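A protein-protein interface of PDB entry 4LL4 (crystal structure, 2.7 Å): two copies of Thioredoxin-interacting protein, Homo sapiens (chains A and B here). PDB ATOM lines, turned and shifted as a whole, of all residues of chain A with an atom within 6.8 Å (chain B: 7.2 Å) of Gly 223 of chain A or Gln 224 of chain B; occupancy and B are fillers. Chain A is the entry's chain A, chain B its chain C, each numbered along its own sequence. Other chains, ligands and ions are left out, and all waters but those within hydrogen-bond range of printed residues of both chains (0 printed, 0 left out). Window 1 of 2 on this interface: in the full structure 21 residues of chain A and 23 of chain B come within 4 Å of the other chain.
The backbone carbonyl oxygen (O) of Asn 222 of chain A sits close to the side-chain amide oxygen (OE1) of Gln 224 of chain A, at 2.6 Å. O of Tyr 219 of chain B lies within hydrogen-bond range of N of Lys 226 of chain B, at 2.8 Å. N of Leu 220 of chain B sits at hydrogen-bond distance from O of Asn 266 of chain B (2.9 Å).
Arg 69 of chain A touches Gln 224 of chain B, but with the chains exchanged Gln 224 of chain A does not touch Arg 69 of chain B (4.4 Å). Leu 220 of chain A touches Gly 223 of chain B, and with the chains exchanged Gly 223 of chain A touches Leu 220 of chain B. Asn 222 of chain A touches Arg 69 of chain B, but with the chains exchanged Arg 69 of chain A does not touch Asn 222 of chain B (5.1 Å). Gly 223 of chain A touches Gln 224 of chain B, and with the chains exchanged Gln 224 of chain A touches Gly 223 of chain B.
Hydrophobic or aromatic side chains of chain A within 4 Å of the printed part of chain B: Tyr 70 and Leu 220. Among the printed residues, 12 pairs touch across the chains. Among the printed residues, no Asp or Glu carboxylate lies within 4 Å of a Lys or Arg side-chain nitrogen of the other chain.
The backbone NH of Glu 71 of chain A is in hydrogen-bond range of the side-chain amide oxygen of Gln 224 of chain B, at 2.8 Å. O of Glu 71 of chain A sits close to NZ of Lys 226 of chain B (3.1 Å). The backbone NH (N) of Gln 224 of chain A is in hydrogen-bond range of the backbone carbonyl oxygen (O) of Gly 223 of chain B, 3.5 Å away. The backbone carbonyl oxygen (O) of Gly 223 of chain A sits close to the backbone carbonyl oxygen (O) of Gly 223 of chain B (3.2 Å).
Gly 223 of chain A touches just these residues of chain B: Leu 220 (3.6 Å), Gly 223 (3.2 Å) and Gln 224 (3.8 Å). Gln 224 of chain B touches four residues of chain A. Of the printed residues of chain A, Arg 69 of chain B touches Asn 222. Of the printed residues of chain B, Arg 69 of chain A touches Gln 224. Of the printed residues of chain A, Gly 223 of chain B touches Leu 220 (3.4 Å), Gly 223 (3.2 Å) and Gln 224 (3.5 Å). Of the printed residues of chain B, Glu 71 of chain A touches Gln 224 (2.8 Å) and Lys 226 (3.0 Å). Printed residues of chain B within 4 Å of Tyr 70 of chain A: Gln 224. Ala 221 of chain A touches none of the printed residues of chain B. Ala 221 of chain B touches none of the printed residues of chain A. The nearest printed residue of chain B that does not touch Gly 223 of chain A is Ala 221 of chain B (4.3 Å). The nearest residue of chain A that does not touch Gln 224 of chain B is Gln 224 of chain A (4.5 Å).
O of Arg 69 of chain A touches OE1 of Gln 224 of chain B (3.8 Å). Gln 224 of chain B touches Tyr 70 of chain A (OE1 to CA, 3.4 Å). CD1 of Leu 220 of chain A touches C of Asn 222 of chain B, at 3.8 Å. Gly 223 of chain B touches Leu 220 of chain A. Asn 222 of chain A touches Arg 69 of chain B (O to O, 3.8 Å). Asn 222 of chain A touches Leu 220 of chain B (C to CD1, 3.4 Å). Leu 220 of chain B touches Gly 223 of chain A. Gly 223 of chain A touches Gln 224 of chain B (CA to C, 3.8 Å).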
ATOM      1  N   LEU A  45      28.352 -17.416  18.516  1.00  0.00           N
ATOM      2  CA  LEU A  45      28.323 -18.360  19.612  1.00  0.00           C
ATOM      3  C   LEU A  45      29.250 -17.840  20.736  1.00  0.00           C
ATOM      4  O   LEU A  45      30.393 -17.401  20.512  1.00  0.00           O
ATOM      5  CB  LEU A  45      28.776 -19.699  19.094  1.00  0.00           C
ATOM      6  CG  LEU A  45      28.668 -20.890  20.039  1.00  0.00           C
ATOM      7  CD1 LEU A  45      27.246 -21.137  20.585  1.00  0.00           C
ATOM      8  CD2 LEU A  45      29.203 -22.135  19.381  1.00  0.00           C
ATOM      9  N   ARG A  69      26.252 -20.960  26.978  1.00  0.00           N
ATOM     10  CA  ARG A  69      25.997 -21.440  25.590  1.00  0.00           C
ATOM     11  C   ARG A  69      25.046 -20.407  25.097  1.00  0.00           C
ATOM     12  O   ARG A  69      23.929 -20.314  25.584  1.00  0.00           O
ATOM     13  CB  ARG A  69      25.299 -22.792  25.497  1.00  0.00           C
ATOM     14  CG  ARG A  69      26.213 -23.964  25.107  1.00  0.00           C
ATOM     15  CD  ARG A  69      25.381 -25.282  24.974  1.00  0.00           C
ATOM     16  NE  ARG A  69      26.191 -26.512  25.004  1.00  0.00           N
ATOM     17  CZ  ARG A  69      25.701 -27.758  24.998  1.00  0.00           C
ATOM     18  NH1 ARG A  69      24.398 -27.987  24.972  1.00  0.00           N
ATOM     19  NH2 ARG A  69      26.529 -28.791  25.013  1.00  0.00           N
ATOM     20  N   TYR A  70      25.507 -19.564  24.193  1.00  0.00           N
ATOM     21  CA  TYR A  70      24.678 -18.479  23.761  1.00  0.00           C
ATOM     22  C   TYR A  70      24.886 -18.337  22.266  1.00  0.00           C
ATOM     23  O   TYR A  70      26.008 -18.351  21.761  1.00  0.00           O
ATOM     24  CB  TYR A  70      24.976 -17.206  24.579  1.00  0.00           C
ATOM     25  CG  TYR A  70      24.251 -16.016  24.054  1.00  0.00           C
ATOM     26  CD1 TYR A  70      23.031 -15.608  24.618  1.00  0.00           C
ATOM     27  CD2 TYR A  70      24.745 -15.331  22.945  1.00  0.00           C
ATOM     28  CE1 TYR A  70      22.343 -14.528  24.099  1.00  0.00           C
ATOM     29  CE2 TYR A  70      24.069 -14.277  22.412  1.00  0.00           C
ATOM     30  CZ  TYR A  70      22.887 -13.871  22.989  1.00  0.00           C
ATOM     31  OH  TYR A  70      22.261 -12.812  22.432  1.00  0.00           O
ATOM     32  N   GLU A  71      23.780 -18.273  21.546  1.00  0.00           N
ATOM     33  CA  GLU A  71      23.858 -18.174  20.099  1.00  0.00           C
ATOM     34  C   GLU A  71      22.760 -17.315  19.613  1.00  0.00           C
ATOM     35  O   GLU A  71      21.667 -17.324  20.178  1.00  0.00           O
ATOM     36  CB  GLU A  71      23.884 -19.531  19.388  1.00  0.00           C
ATOM     37  CG  GLU A  71      23.061 -20.591  20.042  1.00  0.00           C
ATOM     38  CD  GLU A  71      23.359 -21.968  19.492  1.00  0.00           C
ATOM     39  OE1 GLU A  71      24.046 -22.083  18.457  1.00  0.00           O
ATOM     40  OE2 GLU A  71      22.906 -22.956  20.094  1.00  0.00           O
ATOM     41  N   ASP A  72      23.101 -16.525  18.599  1.00  0.00           N
ATOM     42  CA  ASP A  72      22.225 -15.515  18.038  1.00  0.00           C
ATOM     43  C   ASP A  72      22.664 -15.224  16.615  1.00  0.00           C
ATOM     44  O   ASP A  72      23.834 -15.365  16.234  1.00  0.00           O
ATOM     45  CB  ASP A  72      22.289 -14.234  18.894  1.00  0.00           C
ATOM     46  CG  ASP A  72      21.020 -13.312  18.760  1.00  0.00           C
ATOM     47  OD1 ASP A  72      19.860 -13.824  18.717  1.00  0.00           O
ATOM     48  OD2 ASP A  72      21.191 -12.052  18.745  1.00  0.00           O
ATOM     49  N   LEU A 220      19.759 -27.138  29.730  1.00  0.00           N
ATOM     50  CA  LEU A 220      19.060 -26.239  28.818  1.00  0.00           C
ATOM     51  C   LEU A 220      17.688 -26.782  28.372  1.00  0.00           C
ATOM     52  O   LEU A 220      17.631 -27.787  27.607  1.00  0.00           O
ATOM     53  CB  LEU A 220      19.952 -25.928  27.612  1.00  0.00           C
ATOM     54  CG  LEU A 220      21.165 -25.043  27.912  1.00  0.00           C
ATOM     55  CD1 LEU A 220      22.023 -24.875  26.619  1.00  0.00           C
ATOM     56  CD2 LEU A 220      20.781 -23.679  28.639  1.00  0.00           C
ATOM     57  N   ALA A 221      16.607 -26.147  28.861  1.00  0.00           N
ATOM     58  CA  ALA A 221      15.254 -26.509  28.396  1.00  0.00           C
ATOM     59  C   ALA A 221      14.177 -25.410  28.469  1.00  0.00           C
ATOM     60  O   ALA A 221      13.996 -24.749  29.524  1.00  0.00           O
ATOM     61  CB  ALA A 221      14.732 -27.832  29.070  1.00  0.00           C
ATOM     62  N   ASN A 222      13.458 -25.259  27.340  1.00  0.00           N
ATOM     63  CA  ASN A 222      12.250 -24.424  27.238  1.00  0.00           C
ATOM     64  C   ASN A 222      12.479 -22.973  27.668  1.00  0.00           C
ATOM     65  O   ASN A 222      11.704 -22.416  28.492  1.00  0.00           O
ATOM     66  CB  ASN A 222      11.073 -25.050  28.016  1.00  0.00           C
ATOM     67  CG  ASN A 222      10.620 -26.419  27.429  1.00  0.00           C
ATOM     68  OD1 ASN A 222      10.889 -26.745  26.261  1.00  0.00           O
ATOM     69  ND2 ASN A 222       9.922 -27.210  28.249  1.00  0.00           N
ATOM     70  N   GLY A 223      13.549 -22.389  27.094  1.00  0.00           N
ATOM     71  CA  GLY A 223      14.014 -21.029  27.393  1.00  0.00           C
ATOM     72  C   GLY A 223      14.937 -20.874  28.602  1.00  0.00           C
ATOM     73  O   GLY A 223      15.334 -19.742  28.953  1.00  0.00           O
ATOM     74  N   GLN A 224      15.299 -22.014  29.208  1.00  0.00           N
ATOM     75  CA  GLN A 224      15.867 -22.096  30.573  1.00  0.00           C
ATOM     76  C   GLN A 224      17.187 -22.930  30.634  1.00  0.00           C
ATOM     77  O   GLN A 224      17.419 -23.737  29.713  1.00  0.00           O
ATOM     78  CB  GLN A 224      14.770 -22.685  31.470  1.00  0.00           C
ATOM     79  CG  GLN A 224      13.622 -21.721  31.922  1.00  0.00           C
ATOM     80  CD  GLN A 224      13.428 -20.485  31.029  1.00  0.00           C
ATOM     81  OE1 GLN A 224      12.643 -20.522  30.074  1.00  0.00           O
ATOM     82  NE2 GLN A 224      14.148 -19.387  31.334  1.00  0.00           N
ATOM     83  N   THR A 225      18.041 -22.868  31.674  1.00  0.00           N
ATOM     84  CA  THR A 225      17.859 -22.419  33.092  1.00  0.00           C
ATOM     85  C   THR A 225      17.301 -23.459  34.113  1.00  0.00           C
ATOM     86  O   THR A 225      16.677 -23.056  35.116  1.00  0.00           O
ATOM     87  CB  THR A 225      17.137 -21.032  33.281  1.00  0.00           C
ATOM     88  OG1 THR A 225      17.400 -20.551  34.614  1.00  0.00           O
ATOM     89  CG2 THR A 225      15.685 -21.183  33.263  1.00  0.00           C
ATOM     90  N   ARG B  69       6.402 -18.869  29.150  1.00  0.00           N
ATOM     91  CA  ARG B  69       6.133 -20.272  29.399  1.00  0.00           C
ATOM     92  C   ARG B  69       7.229 -20.897  30.247  1.00  0.00           C
ATOM     93  O   ARG B  69       8.334 -21.228  29.765  1.00  0.00           O
ATOM     94  CB  ARG B  69       5.948 -21.085  28.136  1.00  0.00           C
ATOM     95  CG  ARG B  69       5.228 -22.319  28.521  1.00  0.00           C
ATOM     96  CD  ARG B  69       5.302 -23.321  27.490  1.00  0.00           C
ATOM     97  NE  ARG B  69       4.998 -22.752  26.204  1.00  0.00           N
ATOM     98  CZ  ARG B  69       5.606 -23.136  25.100  1.00  0.00           C
ATOM     99  NH1 ARG B  69       6.550 -24.057  25.147  1.00  0.00           N
ATOM    100  NH2 ARG B  69       5.289 -22.586  23.951  1.00  0.00           N
ATOM    101  N   TYR B 219      10.762 -17.741  19.778  1.00  0.00           N
ATOM    102  CA  TYR B 219      10.556 -19.146  20.008  1.00  0.00           C
ATOM    103  C   TYR B 219      11.623 -19.617  20.959  1.00  0.00           C
ATOM    104  O   TYR B 219      12.580 -18.875  21.202  1.00  0.00           O
ATOM    105  CB  TYR B 219      10.558 -19.891  18.669  1.00  0.00           C
ATOM    106  CG  TYR B 219      11.933 -19.900  18.110  1.00  0.00           C
ATOM    107  CD1 TYR B 219      12.461 -18.769  17.460  1.00  0.00           C
ATOM    108  CD2 TYR B 219      12.772 -21.017  18.317  1.00  0.00           C
ATOM    109  CE1 TYR B 219      13.775 -18.774  16.976  1.00  0.00           C
ATOM    110  CE2 TYR B 219      14.082 -21.041  17.820  1.00  0.00           C
ATOM    111  CZ  TYR B 219      14.572 -19.932  17.153  1.00  0.00           C
ATOM    112  OH  TYR B 219      15.865 -20.004  16.684  1.00  0.00           O
ATOM    113  N   LEU B 220      11.441 -20.823  21.506  1.00  0.00           N
ATOM    114  CA  LEU B 220      12.374 -21.454  22.510  1.00  0.00           C
ATOM    115  C   LEU B 220      13.275 -22.460  21.835  1.00  0.00           C
ATOM    116  O   LEU B 220      12.839 -23.526  21.384  1.00  0.00           O
ATOM    117  CB  LEU B 220      11.644 -22.145  23.676  1.00  0.00           C
ATOM    118  CG  LEU B 220      10.722 -21.276  24.531  1.00  0.00           C
ATOM    119  CD1 LEU B 220       9.969 -22.046  25.601  1.00  0.00           C
ATOM    120  CD2 LEU B 220      11.392 -20.023  25.170  1.00  0.00           C
ATOM    121  N   ALA B 221      14.532 -22.077  21.699  1.00  0.00           N
ATOM    122  CA  ALA B 221      15.561 -23.034  21.352  1.00  0.00           C
ATOM    123  C   ALA B 221      16.333 -22.975  22.629  1.00  0.00           C
ATOM    124  O   ALA B 221      15.945 -22.233  23.561  1.00  0.00           O
ATOM    125  CB  ALA B 221      16.400 -22.577  20.165  1.00  0.00           C
ATOM    126  N   ASN B 222      17.419 -23.729  22.696  1.00  0.00           N
ATOM    127  CA  ASN B 222      17.990 -23.976  23.999  1.00  0.00           C
ATOM    128  C   ASN B 222      19.345 -23.329  24.327  1.00  0.00           C
ATOM    129  O   ASN B 222      20.265 -23.246  23.477  1.00  0.00           O
ATOM    130  CB  ASN B 222      17.944 -25.471  24.264  1.00  0.00           C
ATOM    131  CG  ASN B 222      16.720 -26.096  23.635  1.00  0.00           C
ATOM    132  OD1 ASN B 222      15.581 -25.682  23.939  1.00  0.00           O
ATOM    133  ND2 ASN B 222      16.936 -27.041  22.698  1.00  0.00           N
ATOM    134  N   GLY B 223      19.429 -22.834  25.568  1.00  0.00           N
ATOM    135  CA  GLY B 223      18.265 -22.820  26.476  1.00  0.00           C
ATOM    136  C   GLY B 223      17.774 -21.405  26.416  1.00  0.00           C
ATOM    137  O   GLY B 223      17.931 -20.642  27.358  1.00  0.00           O
ATOM    138  N   GLN B 224      17.241 -21.008  25.279  1.00  0.00           N
ATOM    139  CA  GLN B 224      16.906 -19.609  25.160  1.00  0.00           C
ATOM    140  C   GLN B 224      15.626 -19.299  24.394  1.00  0.00           C
ATOM    141  O   GLN B 224      14.991 -20.154  23.754  1.00  0.00           O
ATOM    142  CB  GLN B 224      18.116 -18.767  24.666  1.00  0.00           C
ATOM    143  CG  GLN B 224      19.393 -19.580  24.137  1.00  0.00           C
ATOM    144  CD  GLN B 224      20.443 -18.716  23.362  1.00  0.00           C
ATOM    145  OE1 GLN B 224      21.451 -19.239  22.854  1.00  0.00           O
ATOM    146  NE2 GLN B 224      20.200 -17.415  23.276  1.00  0.00           N
ATOM    147  N   THR B 225      15.235 -18.052  24.565  1.00  0.00           N
ATOM    148  CA  THR B 225      14.239 -17.420  23.754  1.00  0.00           C
ATOM    149  C   THR B 225      15.031 -16.815  22.603  1.00  0.00           C
ATOM    150  O   THR B 225      15.803 -15.860  22.829  1.00  0.00           O
ATOM    151  CB  THR B 225      13.638 -16.266  24.542  1.00  0.00           C
ATOM    152  OG1 THR B 225      13.378 -16.709  25.873  1.00  0.00           O
ATOM    153  CG2 THR B 225      12.355 -15.788  23.919  1.00  0.00           C
ATOM    154  N   LYS B 226      14.884 -17.355  21.391  1.00  0.00           N
ATOM    155  CA  LYS B 226      15.499 -16.672  20.218  1.00  0.00           C
ATOM    156  C   LYS B 226      14.444 -15.863  19.417  1.00  0.00           C
ATOM    157  O   LYS B 226      13.267 -15.866  19.779  1.00  0.00           O
ATOM    158  CB  LYS B 226      16.339 -17.646  19.360  1.00  0.00           C
ATOM    159  CG  LYS B 226      17.016 -18.734  20.201  1.00  0.00           C
ATOM    160  CD  LYS B 226      17.940 -19.572  19.370  1.00  0.00           C
ATOM    161  CE  LYS B 226      19.370 -19.194  19.631  1.00  0.00           C
ATOM    162  NZ  LYS B 226      20.270 -19.539  18.464  1.00  0.00           N
ATOM    163  N   ASN B 266       7.424 -24.826  20.095  1.00  0.00           N
ATOM    164  CA  ASN B 266       8.308 -23.918  20.797  1.00  0.00           C
ATOM    165  C   ASN B 266       8.092 -22.469  20.296  1.00  0.00           C
ATOM    166  O   ASN B 266       8.703 -21.559  20.846  1.00  0.00           O
ATOM    167  CB  ASN B 266       9.778 -24.377  20.661  1.00  0.00           C
ATOM    168  CG  ASN B 266      10.090 -25.045  19.283  1.00  0.00           C
ATOM    169  OD1 ASN B 266       9.275 -25.026  18.328  1.00  0.00           O
ATOM    170  ND2 ASN B 266      11.280 -25.637  19.191  1.00  0.00           N
